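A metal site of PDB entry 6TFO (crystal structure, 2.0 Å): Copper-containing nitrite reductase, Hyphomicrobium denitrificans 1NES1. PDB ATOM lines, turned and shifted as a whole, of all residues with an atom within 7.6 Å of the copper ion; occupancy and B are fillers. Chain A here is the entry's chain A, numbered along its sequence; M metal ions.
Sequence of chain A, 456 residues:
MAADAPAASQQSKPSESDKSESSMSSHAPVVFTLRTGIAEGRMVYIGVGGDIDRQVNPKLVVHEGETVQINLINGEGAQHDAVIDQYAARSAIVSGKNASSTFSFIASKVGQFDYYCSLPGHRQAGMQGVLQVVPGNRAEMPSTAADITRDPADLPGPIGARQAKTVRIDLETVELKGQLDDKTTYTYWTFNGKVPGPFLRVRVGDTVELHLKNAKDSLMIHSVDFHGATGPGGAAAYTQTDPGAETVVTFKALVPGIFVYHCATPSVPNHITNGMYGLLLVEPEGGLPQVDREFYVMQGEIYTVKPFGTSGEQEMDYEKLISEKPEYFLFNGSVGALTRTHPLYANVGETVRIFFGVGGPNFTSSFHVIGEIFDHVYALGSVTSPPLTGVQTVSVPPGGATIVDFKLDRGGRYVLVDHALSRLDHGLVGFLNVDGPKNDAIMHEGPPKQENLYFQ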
ATOM      1  N   THR A 173     -18.719   3.944  18.206  1.00  0.00           N
ATOM      2  CA  THR A 173     -18.456   3.888  19.673  1.00  0.00           C
ATOM      3  C   THR A 173     -17.071   4.498  19.893  1.00  0.00           C
ATOM      4  O   THR A 173     -16.085   3.962  19.312  1.00  0.00           O
ATOM      5  CB  THR A 173     -18.684   2.482  20.212  1.00  0.00           C
ATOM      6  OG1 THR A 173     -17.815   1.539  19.570  1.00  0.00           O
ATOM      7  CG2 THR A 173     -20.116   2.046  20.019  1.00  0.00           C
ATOM      8  N   GLU A 175     -14.454   6.204  22.866  1.00  0.00           N
ATOM      9  CA  GLU A 175     -13.976   6.430  24.256  1.00  0.00           C
ATOM     10  C   GLU A 175     -13.148   7.705  24.216  1.00  0.00           C
ATOM     11  O   GLU A 175     -12.313   7.828  23.311  1.00  0.00           O
ATOM     12  CB  GLU A 175     -13.162   5.229  24.746  1.00  0.00           C
ATOM     13  CG  GLU A 175     -13.893   3.899  24.643  1.00  0.00           C
ATOM     14  CD  GLU A 175     -13.022   2.685  24.943  1.00  0.00           C
ATOM     15  OE1 GLU A 175     -13.556   1.563  24.972  1.00  0.00           O
ATOM     16  OE2 GLU A 175     -11.801   2.858  25.116  1.00  0.00           O
ATOM     17  N   TRP A 189     -17.463   6.992  27.546  1.00  0.00           N
ATOM     18  CA  TRP A 189     -17.742   6.081  26.419  1.00  0.00           C
ATOM     19  C   TRP A 189     -19.068   6.544  25.789  1.00  0.00           C
ATOM     20  O   TRP A 189     -20.057   6.733  26.531  1.00  0.00           O
ATOM     21  CB  TRP A 189     -17.810   4.620  26.901  1.00  0.00           C
ATOM     22  CG  TRP A 189     -16.595   4.161  27.653  1.00  0.00           C
ATOM     23  CD1 TRP A 189     -15.373   4.774  27.679  1.00  0.00           C
ATOM     24  CD2 TRP A 189     -16.459   2.955  28.413  1.00  0.00           C
ATOM     25  NE1 TRP A 189     -14.516   4.039  28.433  1.00  0.00           N
ATOM     26  CE2 TRP A 189     -15.148   2.917  28.902  1.00  0.00           C
ATOM     27  CE3 TRP A 189     -17.332   1.919  28.753  1.00  0.00           C
ATOM     28  CZ2 TRP A 189     -14.674   1.883  29.696  1.00  0.00           C
ATOM     29  CZ3 TRP A 189     -16.872   0.888  29.550  1.00  0.00           C
ATOM     30  CH2 TRP A 189     -15.559   0.878  30.021  1.00  0.00           C
ATOM     31  N   THR A 190     -19.091   6.710  24.466  1.00  0.00           N
ATOM     32  CA  THR A 190     -20.215   7.362  23.748  1.00  0.00           C
ATOM     33  C   THR A 190     -20.536   6.650  22.432  1.00  0.00           C
ATOM     34  O   THR A 190     -19.689   5.918  21.895  1.00  0.00           O
ATOM     35  CB  THR A 190     -19.887   8.821  23.436  1.00  0.00           C
ATOM     36  OG1 THR A 190     -18.867   8.821  22.444  1.00  0.00           O
ATOM     37  CG2 THR A 190     -19.475   9.601  24.672  1.00  0.00           C
ATOM     38  N   PHE A 191     -21.743   6.916  21.942  1.00  0.00           N
ATOM     39  CA  PHE A 191     -22.096   6.816  20.503  1.00  0.00           C
ATOM     40  C   PHE A 191     -21.815   8.195  19.895  1.00  0.00           C
ATOM     41  O   PHE A 191     -22.431   9.171  20.326  1.00  0.00           O
ATOM     42  CB  PHE A 191     -23.531   6.319  20.382  1.00  0.00           C
ATOM     43  CG  PHE A 191     -23.822   4.962  20.990  1.00  0.00           C
ATOM     44  CD1 PHE A 191     -23.384   3.808  20.363  1.00  0.00           C
ATOM     45  CD2 PHE A 191     -24.584   4.847  22.139  1.00  0.00           C
ATOM     46  CE1 PHE A 191     -23.698   2.569  20.895  1.00  0.00           C
ATOM     47  CE2 PHE A 191     -24.882   3.606  22.682  1.00  0.00           C
ATOM     48  CZ  PHE A 191     -24.433   2.460  22.058  1.00  0.00           C
ATOM     49  N   ASN A 214     -16.695   0.485  15.929  1.00  0.00           N
ATOM     50  CA  ASN A 214     -15.938   0.730  17.197  1.00  0.00           C
ATOM     51  C   ASN A 214     -14.602   1.368  16.835  1.00  0.00           C
ATOM     52  O   ASN A 214     -13.825   0.717  16.118  1.00  0.00           O
ATOM     53  CB  ASN A 214     -15.761  -0.544  18.034  1.00  0.00           C
ATOM     54  CG  ASN A 214     -15.286  -0.294  19.452  1.00  0.00           C
ATOM     55  OD1 ASN A 214     -15.157   0.852  19.888  1.00  0.00           O
ATOM     56  ND2 ASN A 214     -15.060  -1.373  20.201  1.00  0.00           N
ATOM     57  N   MET A 220     -12.238  -0.998  24.908  1.00  0.00           N
ATOM     58  CA  MET A 220     -13.323  -1.976  25.178  1.00  0.00           C
ATOM     59  C   MET A 220     -14.053  -2.351  23.884  1.00  0.00           C
ATOM     60  O   MET A 220     -14.163  -1.519  22.951  1.00  0.00           O
ATOM     61  CB  MET A 220     -14.321  -1.414  26.198  1.00  0.00           C
ATOM     62  CG  MET A 220     -13.665  -0.850  27.428  1.00  0.00           C
ATOM     63  SD  MET A 220     -12.462  -1.975  28.158  1.00  0.00           S
ATOM     64  CE  MET A 220     -12.060  -1.050  29.641  1.00  0.00           C
ATOM     65  N   ILE A 221     -14.537  -3.602  23.852  1.00  0.00           N
ATOM     66  CA  ILE A 221     -15.644  -4.046  22.965  1.00  0.00           C
ATOM     67  C   ILE A 221     -16.860  -3.130  23.250  1.00  0.00           C
ATOM     68  O   ILE A 221     -17.061  -2.755  24.424  1.00  0.00           O
ATOM     69  CB  ILE A 221     -15.922  -5.555  23.188  1.00  0.00           C
ATOM     70  CG1 ILE A 221     -14.728  -6.408  22.721  1.00  0.00           C
ATOM     71  CG2 ILE A 221     -17.206  -5.984  22.512  1.00  0.00           C
ATOM     72  CD1 ILE A 221     -14.718  -7.830  23.217  1.00  0.00           C
ATOM     73  N   HIS A 222     -17.598  -2.735  22.216  1.00  0.00           N
ATOM     74  CA  HIS A 222     -18.900  -2.016  22.363  1.00  0.00           C
ATOM     75  C   HIS A 222     -19.991  -2.702  21.529  1.00  0.00           C
ATOM     76  O   HIS A 222     -19.671  -3.502  20.631  1.00  0.00           O
ATOM     77  CB  HIS A 222     -18.743  -0.544  22.005  1.00  0.00           C
ATOM     78  CG  HIS A 222     -17.851   0.159  22.953  1.00  0.00           C
ATOM     79  ND1 HIS A 222     -18.247   0.427  24.235  1.00  0.00           N
ATOM     80  CD2 HIS A 222     -16.580   0.593  22.835  1.00  0.00           C
ATOM     81  CE1 HIS A 222     -17.256   1.024  24.875  1.00  0.00           C
ATOM     82  NE2 HIS A 222     -16.225   1.132  24.033  1.00  0.00           N
ATOM     83  N   SER A 223     -21.238  -2.371  21.833  1.00  0.00           N
ATOM     84  CA  SER A 223     -22.444  -3.014  21.265  1.00  0.00           C
ATOM     85  C   SER A 223     -23.618  -2.031  21.321  1.00  0.00           C
ATOM     86  O   SER A 223     -23.411  -0.871  21.730  1.00  0.00           O
ATOM     87  CB  SER A 223     -22.721  -4.283  22.016  1.00  0.00           C
ATOM     88  OG  SER A 223     -23.048  -3.999  23.360  1.00  0.00           O
ATOM     89  N   VAL A 224     -24.805  -2.464  20.907  1.00  0.00           N
ATOM     90  CA  VAL A 224     -26.045  -1.668  21.098  1.00  0.00           C
ATOM     91  C   VAL A 224     -27.244  -2.613  21.232  1.00  0.00           C
ATOM     92  O   VAL A 224     -27.323  -3.596  20.456  1.00  0.00           O
ATOM     93  CB  VAL A 224     -26.229  -0.631  19.990  1.00  0.00           C
ATOM     94  CG1 VAL A 224     -26.315  -1.297  18.627  1.00  0.00           C
ATOM     95  CG2 VAL A 224     -27.440   0.252  20.262  1.00  0.00           C
ATOM     96  N   HIS A 262     -28.912   1.599  24.302  1.00  0.00           N
ATOM     97  CA  HIS A 262     -27.693   1.632  25.159  1.00  0.00           C
ATOM     98  C   HIS A 262     -26.714   0.550  24.698  1.00  0.00           C
ATOM     99  O   HIS A 262     -27.163  -0.432  24.080  1.00  0.00           O
ATOM    100  CB  HIS A 262     -28.042   1.502  26.667  1.00  0.00           C
ATOM    101  CG  HIS A 262     -28.797   0.268  27.052  1.00  0.00           C
ATOM    102  ND1 HIS A 262     -28.210  -0.976  27.140  1.00  0.00           N
ATOM    103  CD2 HIS A 262     -30.094   0.102  27.402  1.00  0.00           C
ATOM    104  CE1 HIS A 262     -29.118  -1.871  27.498  1.00  0.00           C
ATOM    105  NE2 HIS A 262     -30.287  -1.235  27.649  1.00  0.00           N
ATOM    106  N   CYS A 263     -25.439   0.721  25.011  1.00  0.00           N
ATOM    107  CA  CYS A 263     -24.429  -0.353  24.900  1.00  0.00           C
ATOM    108  C   CYS A 263     -24.865  -1.551  25.765  1.00  0.00           C
ATOM    109  O   CYS A 263     -25.505  -1.333  26.805  1.00  0.00           O
ATOM    110  CB  CYS A 263     -23.047   0.165  25.281  1.00  0.00           C
ATOM    111  SG  CYS A 263     -21.722  -1.052  25.024  1.00  0.00           S
ATOM    112  N   ALA A 264     -24.556  -2.771  25.336  1.00  0.00           N
ATOM    113  CA  ALA A 264     -24.891  -4.012  26.070  1.00  0.00           C
ATOM    114  C   ALA A 264     -23.688  -4.946  26.032  1.00  0.00           C
ATOM    115  O   ALA A 264     -23.901  -6.143  25.818  1.00  0.00           O
ATOM    116  CB  ALA A 264     -26.112  -4.675  25.486  1.00  0.00           C
ATOM    117  N   THR A 265     -22.491  -4.371  26.206  1.00  0.00           N
ATOM    118  CA  THR A 265     -21.209  -5.095  26.488  1.00  0.00           C
ATOM    119  C   THR A 265     -20.950  -5.063  27.993  1.00  0.00           C
ATOM    120  O   THR A 265     -21.001  -3.996  28.611  1.00  0.00           O
ATOM    121  CB  THR A 265     -20.073  -4.494  25.645  1.00  0.00           C
ATOM    122  OG1 THR A 265     -20.438  -4.623  24.277  1.00  0.00           O
ATOM    123  CG2 THR A 265     -18.748  -5.179  25.884  1.00  0.00           C
ATOM    124  N   PRO A 266     -20.682  -6.210  28.664  1.00  0.00           N
ATOM    125  CA  PRO A 266     -20.436  -6.215  30.109  1.00  0.00           C
ATOM    126  C   PRO A 266     -19.201  -5.386  30.487  1.00  0.00           C
ATOM    127  O   PRO A 266     -18.250  -5.366  29.723  1.00  0.00           O
ATOM    128  CB  PRO A 266     -20.194  -7.687  30.434  1.00  0.00           C
ATOM    129  CG  PRO A 266     -20.741  -8.458  29.245  1.00  0.00           C
ATOM    130  CD  PRO A 266     -20.533  -7.548  28.058  1.00  0.00           C
ATOM    131  N   SER A 267     -19.181  -4.675  31.622  1.00  0.00           N
ATOM    132  CA  SER A 267     -20.311  -4.403  32.509  1.00  0.00           C
ATOM    133  C   SER A 267     -21.238  -3.401  31.830  1.00  0.00           C
ATOM    134  O   SER A 267     -20.792  -2.270  31.509  1.00  0.00           O
ATOM    135  CB  SER A 267     -19.831  -3.878  33.844  1.00  0.00           C
ATOM    136  OG  SER A 267     -20.921  -3.497  34.683  1.00  0.00           O
ATOM    137  N   VAL A 268     -22.486  -3.797  31.632  1.00  0.00           N
ATOM    138  CA  VAL A 268     -23.480  -2.937  30.945  1.00  0.00           C
ATOM    139  C   VAL A 268     -23.671  -1.685  31.795  1.00  0.00           C
ATOM    140  O   VAL A 268     -23.577  -0.570  31.277  1.00  0.00           O
ATOM    141  CB  VAL A 268     -24.773  -3.724  30.666  1.00  0.00           C
ATOM    142  CG1 VAL A 268     -25.833  -2.841  29.994  1.00  0.00           C
ATOM    143  CG2 VAL A 268     -24.494  -4.962  29.807  1.00  0.00           C
ATOM    144  N   ASN A 270     -21.590  -0.157  33.593  1.00  0.00           N
ATOM    145  CA  ASN A 270     -20.345   0.627  33.380  1.00  0.00           C
ATOM    146  C   ASN A 270     -20.446   1.386  32.041  1.00  0.00           C
ATOM    147  O   ASN A 270     -20.257   2.610  32.031  1.00  0.00           O
ATOM    148  CB  ASN A 270     -19.102  -0.264  33.415  1.00  0.00           C
ATOM    149  CG  ASN A 270     -17.794   0.493  33.400  1.00  0.00           C
ATOM    150  OD1 ASN A 270     -17.771   1.719  33.505  1.00  0.00           O
ATOM    151  ND2 ASN A 270     -16.704  -0.235  33.307  1.00  0.00           N
ATOM    152  N   HIS A 271     -20.736   0.667  30.959  1.00  0.00           N
ATOM    153  CA  HIS A 271     -20.916   1.233  29.605  1.00  0.00           C
ATOM    154  C   HIS A 271     -22.009   2.312  29.641  1.00  0.00           C
ATOM    155  O   HIS A 271     -21.822   3.366  29.003  1.00  0.00           O
ATOM    156  CB  HIS A 271     -21.200   0.114  28.605  1.00  0.00           C
ATOM    157  CG  HIS A 271     -19.991  -0.716  28.345  1.00  0.00           C
ATOM    158  ND1 HIS A 271     -19.224  -0.558  27.213  1.00  0.00           N
ATOM    159  CD2 HIS A 271     -19.405  -1.697  29.063  1.00  0.00           C
ATOM    160  CE1 HIS A 271     -18.215  -1.409  27.252  1.00  0.00           C
ATOM    161  NE2 HIS A 271     -18.318  -2.120  28.374  1.00  0.00           N
ATOM    162  N   ILE A 272     -23.060   2.098  30.424  1.00  0.00           N
ATOM    163  CA  ILE A 272     -24.194   3.067  30.508  1.00  0.00           C
ATOM    164  C   ILE A 272     -23.745   4.313  31.280  1.00  0.00           C
ATOM    165  O   ILE A 272     -23.824   5.406  30.676  1.00  0.00           O
ATOM    166  CB  ILE A 272     -25.471   2.401  31.056  1.00  0.00           C
ATOM    167  CG1 ILE A 272     -26.058   1.441  30.017  1.00  0.00           C
ATOM    168  CG2 ILE A 272     -26.488   3.454  31.477  1.00  0.00           C
ATOM    169  CD1 ILE A 272     -27.148   0.538  30.552  1.00  0.00           C
ATOM    170  N   ASN A 274     -20.946   5.574  31.752  1.00  0.00           N
ATOM    171  CA  ASN A 274     -19.861   6.257  31.002  1.00  0.00           C
ATOM    172  C   ASN A 274     -20.421   7.065  29.839  1.00  0.00           C
ATOM    173  O   ASN A 274     -19.713   7.979  29.368  1.00  0.00           O
ATOM    174  CB  ASN A 274     -18.790   5.261  30.541  1.00  0.00           C
ATOM    175  CG  ASN A 274     -17.800   4.913  31.632  1.00  0.00           C
ATOM    176  OD1 ASN A 274     -16.840   4.207  31.372  1.00  0.00           O
ATOM    177  ND2 ASN A 274     -18.050   5.354  32.857  1.00  0.00           N
ATOM    178  N   MET A 276     -23.093   5.669  27.227  1.00  0.00           N
ATOM    179  CA  MET A 276     -23.527   4.937  26.014  1.00  0.00           C
ATOM    180  C   MET A 276     -25.046   4.655  26.115  1.00  0.00           C
ATOM    181  O   MET A 276     -25.466   3.494  26.315  1.00  0.00           O
ATOM    182  CB  MET A 276     -22.710   3.650  25.823  1.00  0.00           C
ATOM    183  CG  MET A 276     -21.204   3.908  25.756  1.00  0.00           C
ATOM    184  SD  MET A 276     -20.210   2.551  25.081  1.00  0.00           S
ATOM    185  CE  MET A 276     -20.457   2.856  23.341  1.00  0.00           C
HETATM  186 CU    CU M   1     -19.903   0.100  25.346  1.00  0.00          CU
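Of the 23 residues printed, 4 come within 4 Å of the copper ion.
The copper ion is bound by a ring nitrogen (ND1) of His 222, a ring nitrogen (ND1) of His 271, the side-chain sulfur of Cys 263 and the side-chain sulfur of Met 276.
The copper ion has four donor atoms within binding distance.
SG of Cys 263 lies close to N of Thr 265 (3.6 Å).
NE2 of His 271 sits close to O of Thr 265, at 3.3 Å.
SG of Cys 263 sits close to N of Ser 223 (3.5 Å).
OE1 of Glu 175 is in hydrogen-bond range of NE2 of His 222, 2.9 Å away.
The backbone carbonyl oxygen (O) of Trp 189 lies close to the backbone NH (N) of Met 276, 3.3 Å away.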
